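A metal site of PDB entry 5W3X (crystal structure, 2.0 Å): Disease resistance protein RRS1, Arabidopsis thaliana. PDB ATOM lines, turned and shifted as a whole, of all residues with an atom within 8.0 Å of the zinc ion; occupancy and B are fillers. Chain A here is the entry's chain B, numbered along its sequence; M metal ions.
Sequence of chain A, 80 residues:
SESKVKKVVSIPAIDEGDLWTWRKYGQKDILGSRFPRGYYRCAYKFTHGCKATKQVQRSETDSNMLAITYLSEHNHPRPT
N of Ala 52 lies close to SG of Cys 50 (3.7 Å).
The backbone carbonyl oxygen (O) of Tyr 44 sits at hydrogen-bond distance from the backbone NH (N) of Cys 50, at 3.3 Å.
The backbone carbonyl oxygen of Ala 52 is in hydrogen-bond range of the backbone NH of Cys 42 (3.0 Å).
SG of Cys 42 lies close to N of Tyr 44 (3.2 Å).
The side-chain sulfur of Cys 42 sits close to the backbone carbonyl oxygen of Thr 21 (3.7 Å).
Of the 21 residues printed, 4 come within 4 Å of the zinc ion.
The zinc ion is bound by NE2 of His 76 (2.1 Å), SG of Cys 50 (2.1 Å), ND1 of His 74 (2.2 Å) and SG of Cys 42 (2.3 Å).
The zinc ion has four donor atoms within binding distance.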
ATOM      1  N   TRP A  20      22.920  -0.470  22.062  1.00  0.00           N
ATOM      2  CA  TRP A  20      23.747   0.417  22.873  1.00  0.00           C
ATOM      3  C   TRP A  20      24.924  -0.260  23.571  1.00  0.00           C
ATOM      4  O   TRP A  20      25.070  -1.481  23.521  1.00  0.00           O
ATOM      5  CB  TRP A  20      22.865   1.100  23.908  1.00  0.00           C
ATOM      6  CG  TRP A  20      21.631   1.677  23.318  1.00  0.00           C
ATOM      7  CD1 TRP A  20      20.409   1.081  23.220  1.00  0.00           C
ATOM      8  CD2 TRP A  20      21.491   2.962  22.703  1.00  0.00           C
ATOM      9  NE1 TRP A  20      19.517   1.917  22.603  1.00  0.00           N
ATOM     10  CE2 TRP A  20      20.156   3.082  22.279  1.00  0.00           C
ATOM     11  CE3 TRP A  20      22.371   4.031  22.491  1.00  0.00           C
ATOM     12  CZ2 TRP A  20      19.672   4.230  21.642  1.00  0.00           C
ATOM     13  CZ3 TRP A  20      21.881   5.166  21.854  1.00  0.00           C
ATOM     14  CH2 TRP A  20      20.553   5.258  21.444  1.00  0.00           C
ATOM     15  N   THR A  21      25.760   0.555  24.215  1.00  0.00           N
ATOM     16  CA  THR A  21      26.896   0.054  24.986  1.00  0.00           C
ATOM     17  C   THR A  21      26.737   0.365  26.473  1.00  0.00           C
ATOM     18  O   THR A  21      26.297   1.456  26.846  1.00  0.00           O
ATOM     19  CB  THR A  21      28.215   0.668  24.488  1.00  0.00           C
ATOM     20  OG1 THR A  21      28.096   2.091  24.397  1.00  0.00           O
ATOM     21  CG2 THR A  21      28.572   0.108  23.115  1.00  0.00           C
ATOM     22  N   TRP A  22      27.087  -0.610  27.308  1.00  0.00           N
ATOM     23  CA  TRP A  22      26.784  -0.567  28.737  1.00  0.00           C
ATOM     24  C   TRP A  22      27.979  -0.949  29.622  1.00  0.00           C
ATOM     25  O   TRP A  22      28.837  -1.717  29.210  1.00  0.00           O
ATOM     26  CB  TRP A  22      25.621  -1.506  29.031  1.00  0.00           C
ATOM     27  CG  TRP A  22      24.394  -1.234  28.189  1.00  0.00           C
ATOM     28  CD1 TRP A  22      24.032  -1.894  27.050  1.00  0.00           C
ATOM     29  CD2 TRP A  22      23.363  -0.268  28.444  1.00  0.00           C
ATOM     30  NE1 TRP A  22      22.847  -1.383  26.565  1.00  0.00           N
ATOM     31  CE2 TRP A  22      22.420  -0.385  27.406  1.00  0.00           C
ATOM     32  CE3 TRP A  22      23.152   0.692  29.428  1.00  0.00           C
ATOM     33  CZ2 TRP A  22      21.287   0.410  27.328  1.00  0.00           C
ATOM     34  CZ3 TRP A  22      22.017   1.487  29.360  1.00  0.00           C
ATOM     35  CH2 TRP A  22      21.109   1.338  28.310  1.00  0.00           C
ATOM     36  N   ARG A  41      24.543   0.913  33.392  1.00  0.00           N
ATOM     37  CA  ARG A  41      24.397   2.324  33.022  1.00  0.00           C
ATOM     38  C   ARG A  41      25.142   2.494  31.709  1.00  0.00           C
ATOM     39  O   ARG A  41      25.875   1.582  31.325  1.00  0.00           O
ATOM     40  CB  ARG A  41      24.934   3.229  34.135  1.00  0.00           C
ATOM     41  CG  ARG A  41      26.366   2.903  34.611  1.00  0.00           C
ATOM     42  CD  ARG A  41      27.430   3.718  33.859  1.00  0.00           C
ATOM     43  NE  ARG A  41      28.763   3.542  34.429  1.00  0.00           N
ATOM     44  CZ  ARG A  41      29.895   3.723  33.765  1.00  0.00           C
ATOM     45  NH1 ARG A  41      29.874   4.048  32.485  1.00  0.00           N
ATOM     46  NH2 ARG A  41      31.060   3.549  34.375  1.00  0.00           N
ATOM     47  N   CYS A  42      24.907   3.584  30.978  1.00  0.00           N
ATOM     48  CA  CYS A  42      25.520   3.740  29.652  1.00  0.00           C
ATOM     49  C   CYS A  42      27.045   3.913  29.650  1.00  0.00           C
ATOM     50  O   CYS A  42      27.617   4.538  30.555  1.00  0.00           O
ATOM     51  CB  CYS A  42      24.907   4.937  28.906  1.00  0.00           C
ATOM     52  SG  CYS A  42      25.558   5.090  27.210  1.00  0.00           S
ATOM     53  N   ALA A  43      27.709   3.385  28.636  1.00  0.00           N
ATOM     54  CA  ALA A  43      29.147   3.556  28.508  1.00  0.00           C
ATOM     55  C   ALA A  43      29.544   5.019  28.313  1.00  0.00           C
ATOM     56  O   ALA A  43      30.705   5.383  28.497  1.00  0.00           O
ATOM     57  CB  ALA A  43      29.685   2.714  27.360  1.00  0.00           C
ATOM     58  N   TYR A  44      28.580   5.862  27.937  1.00  0.00           N
ATOM     59  CA  TYR A  44      28.850   7.293  27.732  1.00  0.00           C
ATOM     60  C   TYR A  44      28.230   8.144  28.833  1.00  0.00           C
ATOM     61  O   TYR A  44      27.926   9.322  28.624  1.00  0.00           O
ATOM     62  CB  TYR A  44      28.319   7.736  26.372  1.00  0.00           C
ATOM     63  CG  TYR A  44      28.860   6.916  25.224  1.00  0.00           C
ATOM     64  CD1 TYR A  44      30.128   7.162  24.712  1.00  0.00           C
ATOM     65  CD2 TYR A  44      28.107   5.886  24.671  1.00  0.00           C
ATOM     66  CE1 TYR A  44      30.636   6.396  23.656  1.00  0.00           C
ATOM     67  CE2 TYR A  44      28.604   5.117  23.623  1.00  0.00           C
ATOM     68  CZ  TYR A  44      29.864   5.382  23.120  1.00  0.00           C
ATOM     69  OH  TYR A  44      30.348   4.612  22.090  1.00  0.00           O
ATOM     70  N   LYS A  45      28.086   7.563  30.030  1.00  0.00           N
ATOM     71  CA  LYS A  45      27.580   8.319  31.168  1.00  0.00           C
ATOM     72  C   LYS A  45      28.515   9.468  31.521  1.00  0.00           C
ATOM     73  O   LYS A  45      28.069  10.563  31.852  1.00  0.00           O
ATOM     74  CB  LYS A  45      27.420   7.406  32.385  1.00  0.00           C
ATOM     75  CG  LYS A  45      27.003   8.155  33.653  1.00  0.00           C
ATOM     76  CD  LYS A  45      26.726   7.183  34.792  1.00  0.00           C
ATOM     77  CE  LYS A  45      26.276   7.908  36.044  1.00  0.00           C
ATOM     78  NZ  LYS A  45      25.120   8.805  35.752  1.00  0.00           N
ATOM     79  N   HIS A  48      29.493  11.849  28.016  1.00  0.00           N
ATOM     80  CA  HIS A  48      28.368  12.593  27.454  1.00  0.00           C
ATOM     81  C   HIS A  48      27.266  12.942  28.442  1.00  0.00           C
ATOM     82  O   HIS A  48      26.270  13.573  28.065  1.00  0.00           O
ATOM     83  CB  HIS A  48      27.754  11.796  26.309  1.00  0.00           C
ATOM     84  CG  HIS A  48      28.615  11.751  25.083  1.00  0.00           C
ATOM     85  ND1 HIS A  48      29.712  10.931  24.972  1.00  0.00           N
ATOM     86  CD2 HIS A  48      28.540  12.455  23.919  1.00  0.00           C
ATOM     87  CE1 HIS A  48      30.270  11.119  23.787  1.00  0.00           C
ATOM     88  NE2 HIS A  48      29.580  12.037  23.129  1.00  0.00           N
ATOM     89  N   GLY A  49      27.433  12.546  29.702  1.00  0.00           N
ATOM     90  CA  GLY A  49      26.396  12.769  30.701  1.00  0.00           C
ATOM     91  C   GLY A  49      25.147  11.937  30.483  1.00  0.00           C
ATOM     92  O   GLY A  49      24.109  12.215  31.091  1.00  0.00           O
ATOM     93  N   CYS A  50      25.230  10.911  29.643  1.00  0.00           N
ATOM     94  CA  CYS A  50      24.063  10.079  29.308  1.00  0.00           C
ATOM     95  C   CYS A  50      23.473   9.433  30.561  1.00  0.00           C
ATOM     96  O   CYS A  50      24.210   8.882  31.395  1.00  0.00           O
ATOM     97  CB  CYS A  50      24.427   9.014  28.267  1.00  0.00           C
ATOM     98  SG  CYS A  50      23.031   7.952  27.723  1.00  0.00           S
ATOM     99  N   LYS A  51      22.151   9.504  30.704  1.00  0.00           N
ATOM    100  CA  LYS A  51      21.483   9.061  31.928  1.00  0.00           C
ATOM    101  C   LYS A  51      20.832   7.673  31.796  1.00  0.00           C
ATOM    102  O   LYS A  51      20.219   7.170  32.739  1.00  0.00           O
ATOM    103  CB  LYS A  51      20.427  10.092  32.336  1.00  0.00           C
ATOM    104  CG  LYS A  51      21.015  11.410  32.819  1.00  0.00           C
ATOM    105  CD  LYS A  51      19.917  12.350  33.287  1.00  0.00           C
ATOM    106  CE  LYS A  51      20.504  13.611  33.905  1.00  0.00           C
ATOM    107  NZ  LYS A  51      19.441  14.525  34.412  1.00  0.00           N
ATOM    108  N   ALA A  52      20.977   7.080  30.621  1.00  0.00           N
ATOM    109  CA  ALA A  52      20.322   5.808  30.328  1.00  0.00           C
ATOM    110  C   ALA A  52      20.862   4.668  31.209  1.00  0.00           C
ATOM    111  O   ALA A  52      22.061   4.448  31.288  1.00  0.00           O
ATOM    112  CB  ALA A  52      20.489   5.469  28.854  1.00  0.00           C
ATOM    113  N   THR A  53      19.940   3.974  31.875  1.00  0.00           N
ATOM    114  CA  THR A  53      20.280   2.799  32.672  1.00  0.00           C
ATOM    115  C   THR A  53      19.411   1.611  32.262  1.00  0.00           C
ATOM    116  O   THR A  53      18.368   1.780  31.634  1.00  0.00           O
ATOM    117  CB  THR A  53      20.076   3.054  34.165  1.00  0.00           C
ATOM    118  OG1 THR A  53      18.699   3.300  34.408  1.00  0.00           O
ATOM    119  CG2 THR A  53      20.877   4.267  34.612  1.00  0.00           C
ATOM    120  N   SER A  72      15.355   6.282  31.382  1.00  0.00           N
ATOM    121  CA  SER A  72      15.908   7.487  30.766  1.00  0.00           C
ATOM    122  C   SER A  72      16.412   7.234  29.337  1.00  0.00           C
ATOM    123  O   SER A  72      16.704   6.113  28.949  1.00  0.00           O
ATOM    124  CB  SER A  72      17.046   8.078  31.612  1.00  0.00           C
ATOM    125  N   GLU A  73      16.508   8.312  28.575  1.00  0.00           N
ATOM    126  CA  GLU A  73      16.832   8.202  27.154  1.00  0.00           C
ATOM    127  C   GLU A  73      18.299   8.518  26.929  1.00  0.00           C
ATOM    128  O   GLU A  73      18.881   9.322  27.639  1.00  0.00           O
ATOM    129  CB  GLU A  73      15.943   9.150  26.336  1.00  0.00           C
ATOM    130  CG  GLU A  73      14.436   9.018  26.612  1.00  0.00           C
ATOM    131  CD  GLU A  73      14.001   9.641  27.936  1.00  0.00           C
ATOM    132  OE1 GLU A  73      14.849  10.244  28.628  1.00  0.00           O
ATOM    133  OE2 GLU A  73      12.812   9.509  28.301  1.00  0.00           O
ATOM    134  N   HIS A  74      18.884   7.879  25.918  1.00  0.00           N
ATOM    135  CA  HIS A  74      20.255   8.197  25.543  1.00  0.00           C
ATOM    136  C   HIS A  74      20.310   9.600  24.934  1.00  0.00           C
ATOM    137  O   HIS A  74      19.415   9.982  24.185  1.00  0.00           O
ATOM    138  CB  HIS A  74      20.790   7.173  24.550  1.00  0.00           C
ATOM    139  CG  HIS A  74      20.955   5.797  25.136  1.00  0.00           C
ATOM    140  ND1 HIS A  74      22.160   5.346  25.630  1.00  0.00           N
ATOM    141  CD2 HIS A  74      20.075   4.784  25.292  1.00  0.00           C
ATOM    142  CE1 HIS A  74      22.010   4.112  26.067  1.00  0.00           C
ATOM    143  NE2 HIS A  74      20.753   3.747  25.875  1.00  0.00           N
ATOM    144  N   ASN A  75      21.337  10.365  25.280  1.00  0.00           N
ATOM    145  CA  ASN A  75      21.512  11.708  24.718  1.00  0.00           C
ATOM    146  C   ASN A  75      22.576  11.725  23.625  1.00  0.00           C
ATOM    147  O   ASN A  75      23.356  12.668  23.517  1.00  0.00           O
ATOM    148  CB  ASN A  75      21.864  12.720  25.820  1.00  0.00           C
ATOM    149  CG  ASN A  75      23.219  12.445  26.472  1.00  0.00           C
ATOM    150  OD1 ASN A  75      23.872  11.436  26.193  1.00  0.00           O
ATOM    151  ND2 ASN A  75      23.641  13.356  27.350  1.00  0.00           N
ATOM    152  N   HIS A  76      22.599  10.673  22.818  1.00  0.00           N
ATOM    153  CA  HIS A  76      23.597  10.525  21.766  1.00  0.00           C
ATOM    154  C   HIS A  76      23.143   9.442  20.792  1.00  0.00           C
ATOM    155  O   HIS A  76      22.346   8.582  21.167  1.00  0.00           O
ATOM    156  CB  HIS A  76      24.959  10.192  22.362  1.00  0.00           C
ATOM    157  CG  HIS A  76      24.958   8.941  23.183  1.00  0.00           C
ATOM    158  ND1 HIS A  76      25.219   7.704  22.635  1.00  0.00           N
ATOM    159  CD2 HIS A  76      24.686   8.735  24.493  1.00  0.00           C
ATOM    160  CE1 HIS A  76      25.126   6.779  23.590  1.00  0.00           C
ATOM    161  NE2 HIS A  76      24.812   7.385  24.723  1.00  0.00           N
ATOM    162  N   PRO A  77      23.646   9.478  19.546  1.00  0.00           N
ATOM    163  CA  PRO A  77      23.240   8.435  18.589  1.00  0.00           C
ATOM    164  C   PRO A  77      23.759   7.054  18.974  1.00  0.00           C
ATOM    165  O   PRO A  77      24.626   6.943  19.841  1.00  0.00           O
ATOM    166  CB  PRO A  77      23.879   8.909  17.275  1.00  0.00           C
ATOM    167  CG  PRO A  77      25.000   9.808  17.680  1.00  0.00           C
ATOM    168  CD  PRO A  77      24.513  10.490  18.929  1.00  0.00           C
ATOM    169  N   PRO A  79      25.946   3.812  19.017  1.00  0.00           N
ATOM    170  CA  PRO A  79      27.385   3.614  18.823  1.00  0.00           C
ATOM    171  C   PRO A  79      27.727   2.839  17.544  1.00  0.00           C
ATOM    172  O   PRO A  79      27.840   1.617  17.569  1.00  0.00           O
ATOM    173  CB  PRO A  79      27.803   2.810  20.066  1.00  0.00           C
ATOM    174  CG  PRO A  79      26.544   2.183  20.554  1.00  0.00           C
ATOM    175  CD  PRO A  79      25.465   3.167  20.249  1.00  0.00           C
HETATM  176 ZN    ZN M   1      23.899   6.478  26.425  1.00  0.00          ZN
